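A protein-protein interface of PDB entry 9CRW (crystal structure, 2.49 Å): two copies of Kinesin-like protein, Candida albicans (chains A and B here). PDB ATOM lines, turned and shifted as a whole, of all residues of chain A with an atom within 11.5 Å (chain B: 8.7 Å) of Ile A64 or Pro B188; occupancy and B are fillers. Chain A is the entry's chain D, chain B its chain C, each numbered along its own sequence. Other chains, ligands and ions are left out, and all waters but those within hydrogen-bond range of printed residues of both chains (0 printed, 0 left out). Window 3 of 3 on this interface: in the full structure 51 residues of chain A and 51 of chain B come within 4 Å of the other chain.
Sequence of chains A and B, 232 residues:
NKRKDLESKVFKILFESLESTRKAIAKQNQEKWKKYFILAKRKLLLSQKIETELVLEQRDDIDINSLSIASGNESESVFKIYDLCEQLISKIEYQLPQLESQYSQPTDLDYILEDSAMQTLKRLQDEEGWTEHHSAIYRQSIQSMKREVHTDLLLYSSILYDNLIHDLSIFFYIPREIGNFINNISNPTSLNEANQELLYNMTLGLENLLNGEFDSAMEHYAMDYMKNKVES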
ATOM      1  N   ARG A  59      21.016 -11.899  16.766  1.00  0.00           N
ATOM      2  CA  ARG A  59      22.115 -11.021  16.385  1.00  0.00           C
ATOM      3  C   ARG A  59      21.686 -10.113  15.228  1.00  0.00           C
ATOM      4  O   ARG A  59      21.510 -10.572  14.093  1.00  0.00           O
ATOM      5  CB  ARG A  59      23.325 -11.866  16.005  1.00  0.00           C
ATOM      6  CG  ARG A  59      24.637 -11.109  16.032  1.00  0.00           C
ATOM      7  CD  ARG A  59      25.429 -11.341  14.769  1.00  0.00           C
ATOM      8  NE  ARG A  59      26.795 -10.860  14.908  1.00  0.00           N
ATOM      9  CZ  ARG A  59      27.845 -11.657  15.040  1.00  0.00           C
ATOM     10  NH1 ARG A  59      27.714 -12.980  15.038  1.00  0.00           N
ATOM     11  NH2 ARG A  59      29.058 -11.118  15.169  1.00  0.00           N
ATOM     12  N   ASP A  60      21.532  -8.817  15.505  1.00  0.00           N
ATOM     13  CA  ASP A  60      21.218  -7.833  14.464  1.00  0.00           C
ATOM     14  C   ASP A  60      22.008  -6.559  14.764  1.00  0.00           C
ATOM     15  O   ASP A  60      21.514  -5.651  15.442  1.00  0.00           O
ATOM     16  CB  ASP A  60      19.728  -7.564  14.389  1.00  0.00           C
ATOM     17  CG  ASP A  60      19.382  -6.453  13.407  1.00  0.00           C
ATOM     18  OD1 ASP A  60      19.893  -6.492  12.262  1.00  0.00           O
ATOM     19  OD2 ASP A  60      18.598  -5.543  13.775  1.00  0.00           O
ATOM     20  N   ASP A  61      23.233  -6.489  14.245  1.00  0.00           N
ATOM     21  CA  ASP A  61      24.147  -5.408  14.606  1.00  0.00           C
ATOM     22  C   ASP A  61      23.730  -4.087  13.950  1.00  0.00           C
ATOM     23  O   ASP A  61      23.374  -4.046  12.767  1.00  0.00           O
ATOM     24  CB  ASP A  61      25.581  -5.782  14.222  1.00  0.00           C
ATOM     25  CG  ASP A  61      26.110  -7.016  14.995  1.00  0.00           C
ATOM     26  OD1 ASP A  61      26.768  -7.889  14.375  1.00  0.00           O
ATOM     27  OD2 ASP A  61      25.859  -7.112  16.230  1.00  0.00           O
ATOM     28  N   ILE A  62      23.745  -3.006  14.722  1.00  0.00           N
ATOM     29  CA  ILE A  62      23.490  -1.670  14.194  1.00  0.00           C
ATOM     30  C   ILE A  62      24.795  -0.882  14.231  1.00  0.00           C
ATOM     31  O   ILE A  62      25.486  -0.856  15.262  1.00  0.00           O
ATOM     32  CB  ILE A  62      22.372  -0.956  14.973  1.00  0.00           C
ATOM     33  CG1 ILE A  62      21.020  -1.627  14.671  1.00  0.00           C
ATOM     34  CG2 ILE A  62      22.340   0.520  14.628  1.00  0.00           C
ATOM     35  CD1 ILE A  62      20.866  -2.075  13.198  1.00  0.00           C
ATOM     36  N   ASP A  63      25.145  -0.256  13.103  1.00  0.00           N
ATOM     37  CA  ASP A  63      26.376   0.531  13.036  1.00  0.00           C
ATOM     38  C   ASP A  63      26.300   1.747  13.948  1.00  0.00           C
ATOM     39  O   ASP A  63      25.253   2.397  14.082  1.00  0.00           O
ATOM     40  CB  ASP A  63      26.671   0.980  11.609  1.00  0.00           C
ATOM     41  CG  ASP A  63      27.173  -0.148  10.740  1.00  0.00           C
ATOM     42  OD1 ASP A  63      27.958  -0.994  11.241  1.00  0.00           O
ATOM     43  OD2 ASP A  63      26.775  -0.187   9.554  1.00  0.00           O
ATOM     44  N   ILE A  64      27.432   2.051  14.584  1.00  0.00           N
ATOM     45  CA  ILE A  64      27.463   3.135  15.555  1.00  0.00           C
ATOM     46  C   ILE A  64      27.487   4.477  14.824  1.00  0.00           C
ATOM     47  O   ILE A  64      27.726   4.574  13.612  1.00  0.00           O
ATOM     48  CB  ILE A  64      28.651   2.982  16.532  1.00  0.00           C
ATOM     49  CG1 ILE A  64      28.269   3.449  17.943  1.00  0.00           C
ATOM     50  CG2 ILE A  64      29.825   3.836  16.104  1.00  0.00           C
ATOM     51  CD1 ILE A  64      27.473   2.460  18.788  1.00  0.00           C
ATOM     52  N   ASN A  65      27.177   5.526  15.556  1.00  0.00           N
ATOM     53  CA  ASN A  65      27.219   6.848  14.971  1.00  0.00           C
ATOM     54  C   ASN A  65      28.520   7.553  15.323  1.00  0.00           C
ATOM     55  O   ASN A  65      29.165   7.281  16.341  1.00  0.00           O
ATOM     56  CB  ASN A  65      26.032   7.690  15.438  1.00  0.00           C
ATOM     57  CG  ASN A  65      25.306   8.298  14.279  1.00  0.00           C
ATOM     58  OD1 ASN A  65      25.935   8.669  13.287  1.00  0.00           O
ATOM     59  ND2 ASN A  65      23.982   8.341  14.353  1.00  0.00           N
ATOM     60  N   SER A  66      28.885   8.489  14.451  1.00  0.00           N
ATOM     61  CA  SER A  66      29.879   9.507  14.780  1.00  0.00           C
ATOM     62  C   SER A  66      29.562  10.215  16.099  1.00  0.00           C
ATOM     63  O   SER A  66      30.474  10.713  16.771  1.00  0.00           O
ATOM     64  CB  SER A  66      29.927  10.512  13.637  1.00  0.00           C
ATOM     65  OG  SER A  66      31.030  11.348  13.764  1.00  0.00           O
ATOM     66  N   LEU A  67      28.276  10.254  16.484  1.00  0.00           N
ATOM     67  CA  LEU A  67      27.745  10.987  17.626  1.00  0.00           C
ATOM     68  C   LEU A  67      27.671  10.151  18.897  1.00  0.00           C
ATOM     69  O   LEU A  67      27.411  10.704  19.974  1.00  0.00           O
ATOM     70  CB  LEU A  67      26.346  11.513  17.287  1.00  0.00           C
ATOM     71  CG  LEU A  67      26.291  12.199  15.925  1.00  0.00           C
ATOM     72  CD1 LEU A  67      24.896  12.641  15.538  1.00  0.00           C
ATOM     73  CD2 LEU A  67      27.197  13.384  15.988  1.00  0.00           C
ATOM     74  N   SER A  68      27.899   8.842  18.798  1.00  0.00           N
ATOM     75  CA  SER A  68      27.694   7.962  19.939  1.00  0.00           C
ATOM     76  C   SER A  68      28.597   8.361  21.095  1.00  0.00           C
ATOM     77  O   SER A  68      29.811   8.553  20.932  1.00  0.00           O
ATOM     78  CB  SER A  68      27.926   6.505  19.537  1.00  0.00           C
ATOM     79  OG  SER A  68      26.789   6.029  18.805  1.00  0.00           O
ATOM     80  N   ILE A  69      27.966   8.526  22.259  1.00  0.00           N
ATOM     81  CA  ILE A  69      28.633   8.954  23.481  1.00  0.00           C
ATOM     82  C   ILE A  69      29.077   7.763  24.329  1.00  0.00           C
ATOM     83  O   ILE A  69      29.927   7.933  25.223  1.00  0.00           O
ATOM     84  CB  ILE A  69      27.703   9.904  24.277  1.00  0.00           C
ATOM     85  CG1 ILE A  69      28.492  10.894  25.150  1.00  0.00           C
ATOM     86  CG2 ILE A  69      26.678   9.116  25.088  1.00  0.00           C
ATOM     87  CD1 ILE A  69      27.638  12.044  25.727  1.00  0.00           C
ATOM     88  N   ALA A  70      28.577   6.560  24.030  1.00  0.00           N
ATOM     89  CA  ALA A  70      28.745   5.383  24.870  1.00  0.00           C
ATOM     90  C   ALA A  70      30.217   5.059  25.114  1.00  0.00           C
ATOM     91  O   ALA A  70      31.115   5.498  24.393  1.00  0.00           O
ATOM     92  CB  ALA A  70      28.062   4.172  24.233  1.00  0.00           C
ATOM     93  N   SER A  71      30.447   4.268  26.158  1.00  0.00           N
ATOM     94  CA  SER A  71      31.775   3.818  26.544  1.00  0.00           C
ATOM     95  C   SER A  71      31.669   2.354  26.938  1.00  0.00           C
ATOM     96  O   SER A  71      30.569   1.824  27.126  1.00  0.00           O
ATOM     97  CB  SER A  71      32.342   4.671  27.698  1.00  0.00           C
ATOM     98  OG  SER A  71      33.586   4.174  28.173  1.00  0.00           O
ATOM     99  N   GLY A  72      32.812   1.692  27.048  1.00  0.00           N
ATOM    100  CA  GLY A  72      32.870   0.373  27.644  1.00  0.00           C
ATOM    101  C   GLY A  72      33.301  -0.700  26.656  1.00  0.00           C
ATOM    102  O   GLY A  72      33.397  -0.487  25.448  1.00  0.00           O
ATOM    103  N   ASN A  73      33.563  -1.878  27.220  1.00  0.00           N
ATOM    104  CA  ASN A  73      34.041  -3.038  26.485  1.00  0.00           C
ATOM    105  C   ASN A  73      32.931  -4.028  26.176  1.00  0.00           C
ATOM    106  O   ASN A  73      33.215  -5.124  25.673  1.00  0.00           O
ATOM    107  CB  ASN A  73      35.149  -3.737  27.276  1.00  0.00           C
ATOM    108  CG  ASN A  73      36.509  -3.613  26.611  1.00  0.00           C
ATOM    109  OD1 ASN A  73      36.640  -3.008  25.545  1.00  0.00           O
ATOM    110  ND2 ASN A  73      37.532  -4.182  27.244  1.00  0.00           N
ATOM    111  N   GLU A  74      31.678  -3.670  26.464  1.00  0.00           N
ATOM    112  CA  GLU A  74      30.599  -4.653  26.430  1.00  0.00           C
ATOM    113  C   GLU A  74      30.422  -5.253  25.035  1.00  0.00           C
ATOM    114  O   GLU A  74      30.186  -6.463  24.896  1.00  0.00           O
ATOM    115  CB  GLU A  74      29.295  -4.005  26.930  1.00  0.00           C
ATOM    116  CG  GLU A  74      28.759  -2.843  26.063  1.00  0.00           C
ATOM    117  CD  GLU A  74      28.887  -1.477  26.740  1.00  0.00           C
ATOM    118  OE1 GLU A  74      27.876  -0.991  27.310  1.00  0.00           O
ATOM    119  OE2 GLU A  74      30.005  -0.903  26.703  1.00  0.00           O
ATOM    120  N   SER A  75      30.579  -4.438  23.991  1.00  0.00           N
ATOM    121  CA  SER A  75      30.429  -4.948  22.634  1.00  0.00           C
ATOM    122  C   SER A  75      31.486  -6.011  22.297  1.00  0.00           C
ATOM    123  O   SER A  75      31.185  -6.977  21.584  1.00  0.00           O
ATOM    124  CB  SER A  75      30.473  -3.781  21.647  1.00  0.00           C
ATOM    125  OG  SER A  75      30.029  -4.175  20.360  1.00  0.00           O
ATOM    126  N   GLU A  76      32.720  -5.866  22.813  1.00  0.00           N
ATOM    127  CA  GLU A  76      33.756  -6.884  22.588  1.00  0.00           C
ATOM    128  C   GLU A  76      33.361  -8.215  23.224  1.00  0.00           C
ATOM    129  O   GLU A  76      33.478  -9.283  22.598  1.00  0.00           O
ATOM    130  CB  GLU A  76      35.125  -6.420  23.128  1.00  0.00           C
ATOM    131  CG  GLU A  76      36.298  -7.455  22.925  1.00  0.00           C
ATOM    132  CD  GLU A  76      37.525  -7.276  23.861  1.00  0.00           C
ATOM    133  OE1 GLU A  76      37.555  -6.327  24.681  1.00  0.00           O
ATOM    134  OE2 GLU A  76      38.468  -8.102  23.768  1.00  0.00           O
ATOM    135  N   VAL A  78      30.351  -9.250  23.883  1.00  0.00           N
ATOM    136  CA  VAL A  78      29.227  -9.826  23.153  1.00  0.00           C
ATOM    137  C   VAL A  78      29.696 -10.504  21.869  1.00  0.00           C
ATOM    138  O   VAL A  78      29.228 -11.603  21.515  1.00  0.00           O
ATOM    139  CB  VAL A  78      28.181  -8.734  22.880  1.00  0.00           C
ATOM    140  CG1 VAL A  78      27.130  -9.221  21.897  1.00  0.00           C
ATOM    141  CG2 VAL A  78      27.554  -8.318  24.184  1.00  0.00           C
ATOM    142  N   PHE A  79      30.608  -9.862  21.136  1.00  0.00           N
ATOM    143  CA  PHE A  79      31.082 -10.492  19.912  1.00  0.00           C
ATOM    144  C   PHE A  79      31.839 -11.779  20.208  1.00  0.00           C
ATOM    145  O   PHE A  79      31.680 -12.771  19.478  1.00  0.00           O
ATOM    146  CB  PHE A  79      31.909  -9.505  19.101  1.00  0.00           C
ATOM    147  CG  PHE A  79      31.065  -8.590  18.274  1.00  0.00           C
ATOM    148  CD1 PHE A  79      30.083  -7.801  18.879  1.00  0.00           C
ATOM    149  CD2 PHE A  79      31.202  -8.547  16.891  1.00  0.00           C
ATOM    150  CE1 PHE A  79      29.271  -6.963  18.126  1.00  0.00           C
ATOM    151  CE2 PHE A  79      30.394  -7.708  16.120  1.00  0.00           C
ATOM    152  CZ  PHE A  79      29.426  -6.915  16.738  1.00  0.00           C
ATOM    153  N   TYR A  82      29.201 -14.420  20.666  1.00  0.00           N
ATOM    154  CA  TYR A  82      28.679 -14.888  19.377  1.00  0.00           C
ATOM    155  C   TYR A  82      29.664 -15.850  18.717  1.00  0.00           C
ATOM    156  O   TYR A  82      29.273 -16.869  18.115  1.00  0.00           O
ATOM    157  CB  TYR A  82      28.382 -13.708  18.445  1.00  0.00           C
ATOM    158  CG  TYR A  82      27.135 -12.918  18.804  1.00  0.00           C
ATOM    159  CD1 TYR A  82      25.970 -13.548  19.204  1.00  0.00           C
ATOM    160  CD2 TYR A  82      27.134 -11.533  18.741  1.00  0.00           C
ATOM    161  CE1 TYR A  82      24.824 -12.817  19.532  1.00  0.00           C
ATOM    162  CE2 TYR A  82      26.013 -10.799  19.068  1.00  0.00           C
ATOM    163  CZ  TYR A  82      24.861 -11.441  19.462  1.00  0.00           C
ATOM    164  OH  TYR A  82      23.748 -10.697  19.786  1.00  0.00           O
ATOM    165  N   ILE B 182      21.796  -9.393  25.032  1.00  0.00           N
ATOM    166  CA  ILE B 182      23.186  -9.063  24.725  1.00  0.00           C
ATOM    167  C   ILE B 182      23.262  -8.339  23.392  1.00  0.00           C
ATOM    168  O   ILE B 182      24.112  -7.449  23.215  1.00  0.00           O
ATOM    169  CB  ILE B 182      24.127 -10.285  24.772  1.00  0.00           C
ATOM    170  CG1 ILE B 182      24.011 -11.157  23.515  1.00  0.00           C
ATOM    171  CG2 ILE B 182      23.930 -11.088  26.063  1.00  0.00           C
ATOM    172  CD1 ILE B 182      25.025 -12.313  23.496  1.00  0.00           C
ATOM    173  N   ASN B 183      22.339  -8.636  22.459  1.00  0.00           N
ATOM    174  CA  ASN B 183      22.397  -7.929  21.184  1.00  0.00           C
ATOM    175  C   ASN B 183      22.062  -6.458  21.344  1.00  0.00           C
ATOM    176  O   ASN B 183      22.525  -5.640  20.543  1.00  0.00           O
ATOM    177  CB  ASN B 183      21.474  -8.549  20.145  1.00  0.00           C
ATOM    178  CG  ASN B 183      21.467  -7.763  18.814  1.00  0.00           C
ATOM    179  OD1 ASN B 183      22.456  -7.751  18.067  1.00  0.00           O
ATOM    180  ND2 ASN B 183      20.351  -7.105  18.517  1.00  0.00           N
ATOM    181  N   ASN B 184      21.273  -6.070  22.344  1.00  0.00           N
ATOM    182  CA  ASN B 184      21.047  -4.632  22.426  1.00  0.00           C
ATOM    183  C   ASN B 184      21.739  -3.965  23.618  1.00  0.00           C
ATOM    184  O   ASN B 184      21.561  -2.760  23.831  1.00  0.00           O
ATOM    185  CB  ASN B 184      19.541  -4.298  22.357  1.00  0.00           C
ATOM    186  CG  ASN B 184      18.773  -4.771  23.537  1.00  0.00           C
ATOM    187  OD1 ASN B 184      19.282  -4.786  24.661  1.00  0.00           O
ATOM    188  ND2 ASN B 184      17.512  -5.155  23.296  1.00  0.00           N
ATOM    189  N   ILE B 185      22.555  -4.691  24.383  1.00  0.00           N
ATOM    190  CA  ILE B 185      23.615  -3.973  25.103  1.00  0.00           C
ATOM    191  C   ILE B 185      24.787  -3.679  24.165  1.00  0.00           C
ATOM    192  O   ILE B 185      25.380  -2.600  24.228  1.00  0.00           O
ATOM    193  CB  ILE B 185      24.100  -4.715  26.364  1.00  0.00           C
ATOM    194  CG1 ILE B 185      24.898  -5.966  26.005  1.00  0.00           C
ATOM    195  CG2 ILE B 185      22.976  -4.990  27.323  1.00  0.00           C
ATOM    196  CD1 ILE B 185      26.435  -5.732  26.095  1.00  0.00           C
ATOM    197  N   SER B 186      25.106  -4.616  23.255  1.00  0.00           N
ATOM    198  CA  SER B 186      26.165  -4.396  22.277  1.00  0.00           C
ATOM    199  C   SER B 186      25.851  -3.222  21.336  1.00  0.00           C
ATOM    200  O   SER B 186      26.758  -2.474  20.940  1.00  0.00           O
ATOM    201  CB  SER B 186      26.382  -5.686  21.478  1.00  0.00           C
ATOM    202  OG  SER B 186      27.348  -5.542  20.429  1.00  0.00           O
ATOM    203  N   ASN B 187      24.586  -3.073  20.941  1.00  0.00           N
ATOM    204  CA  ASN B 187      24.134  -2.031  20.040  1.00  0.00           C
ATOM    205  C   ASN B 187      24.107  -0.686  20.777  1.00  0.00           C
ATOM    206  O   ASN B 187      24.231  -0.638  22.011  1.00  0.00           O
ATOM    207  CB  ASN B 187      22.754  -2.423  19.471  1.00  0.00           C
ATOM    208  CG  ASN B 187      22.833  -3.376  18.238  1.00  0.00           C
ATOM    209  OD1 ASN B 187      23.711  -3.248  17.387  1.00  0.00           O
ATOM    210  ND2 ASN B 187      21.878  -4.311  18.139  1.00  0.00           N
ATOM    211  N   PRO B 188      23.951   0.441  20.054  1.00  0.00           N
ATOM    212  CA  PRO B 188      23.856   1.754  20.741  1.00  0.00           C
ATOM    213  C   PRO B 188      22.758   1.826  21.796  1.00  0.00           C
ATOM    214  O   PRO B 188      22.786   2.738  22.643  1.00  0.00           O
ATOM    215  CB  PRO B 188      23.593   2.743  19.603  1.00  0.00           C
ATOM    216  CG  PRO B 188      23.932   2.031  18.327  1.00  0.00           C
ATOM    217  CD  PRO B 188      23.873   0.562  18.585  1.00  0.00           C
ATOM    218  N   THR B 189      21.793   0.900  21.767  1.00  0.00           N
ATOM    219  CA  THR B 189      20.680   0.866  22.714  1.00  0.00           C
ATOM    220  C   THR B 189      21.183   0.902  24.155  1.00  0.00           C
ATOM    221  O   THR B 189      22.209   0.299  24.486  1.00  0.00           O
ATOM    222  CB  THR B 189      19.842  -0.399  22.463  1.00  0.00           C
ATOM    223  OG1 THR B 189      19.428  -0.435  21.086  1.00  0.00           O
ATOM    224  CG2 THR B 189      18.617  -0.474  23.394  1.00  0.00           C
ATOM    225  N   SER B 190      20.443   1.612  25.016  1.00  0.00           N
ATOM    226  CA  SER B 190      20.890   1.907  26.374  1.00  0.00           C
ATOM    227  C   SER B 190      20.911   0.643  27.235  1.00  0.00           C
ATOM    228  O   SER B 190      20.696  -0.477  26.768  1.00  0.00           O
ATOM    229  CB  SER B 190      19.996   2.970  27.017  1.00  0.00           C
ATOM    230  OG  SER B 190      20.384   3.227  28.359  1.00  0.00           O
ATOM    231  N   LEU B 191      21.185   0.834  28.522  1.00  0.00           N
ATOM    232  CA  LEU B 191      21.187  -0.267  29.474  1.00  0.00           C
ATOM    233  C   LEU B 191      19.817  -0.494  30.098  1.00  0.00           C
ATOM    234  O   LEU B 191      19.464  -1.640  30.420  1.00  0.00           O
ATOM    235  CB  LEU B 191      22.228   0.001  30.568  1.00  0.00           C
ATOM    236  CG  LEU B 191      22.463  -1.132  31.554  1.00  0.00           C
ATOM    237  CD1 LEU B 191      22.691  -2.368  30.733  1.00  0.00           C
ATOM    238  CD2 LEU B 191      23.655  -0.843  32.456  1.00  0.00           C
ATOM    239  N   GLU B 193      16.834   0.357  28.451  1.00  0.00           N
ATOM    240  CA  GLU B 193      16.011  -0.217  27.397  1.00  0.00           C
ATOM    241  C   GLU B 193      16.255  -1.712  27.315  1.00  0.00           C
ATOM    242  O   GLU B 193      15.308  -2.497  27.188  1.00  0.00           O
ATOM    243  CB  GLU B 193      16.286   0.473  26.067  1.00  0.00           C
ATOM    244  CG  GLU B 193      15.604   1.828  25.953  1.00  0.00           C
ATOM    245  CD  GLU B 193      16.509   2.889  25.348  1.00  0.00           C
ATOM    246  OE1 GLU B 193      17.635   2.545  24.907  1.00  0.00           O
ATOM    247  OE2 GLU B 193      16.098   4.069  25.323  1.00  0.00           O
ATOM    248  N   ALA B 194      17.512  -2.128  27.485  1.00  0.00           N
ATOM    249  CA  ALA B 194      17.822  -3.550  27.573  1.00  0.00           C
ATOM    250  C   ALA B 194      17.106  -4.199  28.756  1.00  0.00           C
ATOM    251  O   ALA B 194      16.380  -5.189  28.591  1.00  0.00           O
ATOM    252  CB  ALA B 194      19.333  -3.755  27.671  1.00  0.00           C
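The side-chain hydroxyl (OG) of Ser B186 is in hydrogen-bond range of the side-chain hydroxyl (OG) of Ser A75, 3.0 Å away. The side-chain amide oxygen (OD1) of Asn B183 lies within hydrogen-bond range of the backbone NH (N) of Asp A60, at 2.9 Å. N of Ile A62 sits at hydrogen-bond distance from OD1 of Asn B187. The side-chain amide nitrogen of Asn B187 sits at hydrogen-bond distance from the backbone carbonyl oxygen of Asp A60, 3.0 Å away.
The backbone carbonyl oxygen of Asn B183 is in hydrogen-bond range of the side-chain amide nitrogen of Asn B187 (2.8 Å). NE of Arg A59 lies within salt-bridge range of OD1 of Asp A61 (3.0 Å).
Asn B183 touches Arg A59 (OD1 to CA, 3.7 Å). Asp A61 touches Asn B187. Ile A64 touches Pro B188. Glu A74 touches Ile B185. O of Ile B182 touches CG2 of Val A78 (3.7 Å). CD1 of Ile B185 touches CG2 of Val A78, at 3.4 Å. CB of Ser B186 touches CG1 of Val A78 (3.6 Å). Ser B186 touches Phe A79 (OG to CE1, 3.3 Å). CG1 of Ile B182 touches OH of Tyr A82 (3.8 Å). Tyr A82 touches Asn B183 (OH to CB, 3.1 Å).
Of the printed residues of chain B, Ile A62 touches Asn B187 (2.7 Å) and Pro B188 (3.96 Å). Of the printed residues of chain B, Ile A64 touches Pro B188. Gly A72 touches none of the printed residues of chain B. Asn A73 touches none of the printed residues of chain B. Of the printed residues of chain B, Ser A75 touches Ser B186. Printed residues of chain B within 4 Å of Phe A79: Ser B186 (3.3 Å). Of the printed residues of chain B, Tyr A82 touches Ile B182 and Asn B183. Of the printed residues of chain A, Asn B183 touches Arg A59, Asp A60, Asp A61 and Tyr A82. Of the printed residues of chain A, Ser B186 touches Ser A75, Val A78 and Phe A79. No residue of chain A comes within 4 Å of Ser B190. The nearest residue of chain B that does not touch Ile A64 is Asn B187 (5.0 Å). The nearest residue of chain A that does not touch Pro B188 is Asp A63 (4.5 Å). The nearest printed residue of chain B that does not touch Tyr A82 is Ser B186 (5.6 Å).
Of the 21 printed residues of chain A, 10 touch a printed residue of chain B. Printed residues of chain A that touch a printed residue of chain B: Arg A59, Asp A60, Asp A61, Ile A62, Ile A64, Glu A74, Ser A75, Val A78, Phe A79 and Tyr A82. Hydrophobic or aromatic side chains of chain A that line the printed part of chain B: Ile A62, Ile A64, Val A78, Phe A79 and Tyr A82. Printed residues of chain B that touch a printed residue of chain A: Ile B182, Asn B183, Ile B185, Ser B186, Asn B187 and Pro B188. Hydrophobic or aromatic side chains of chain B within 4 Å of the printed part of chain A: Ile B182, Ile B185 and Pro B188.
No position is printed for both chains.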
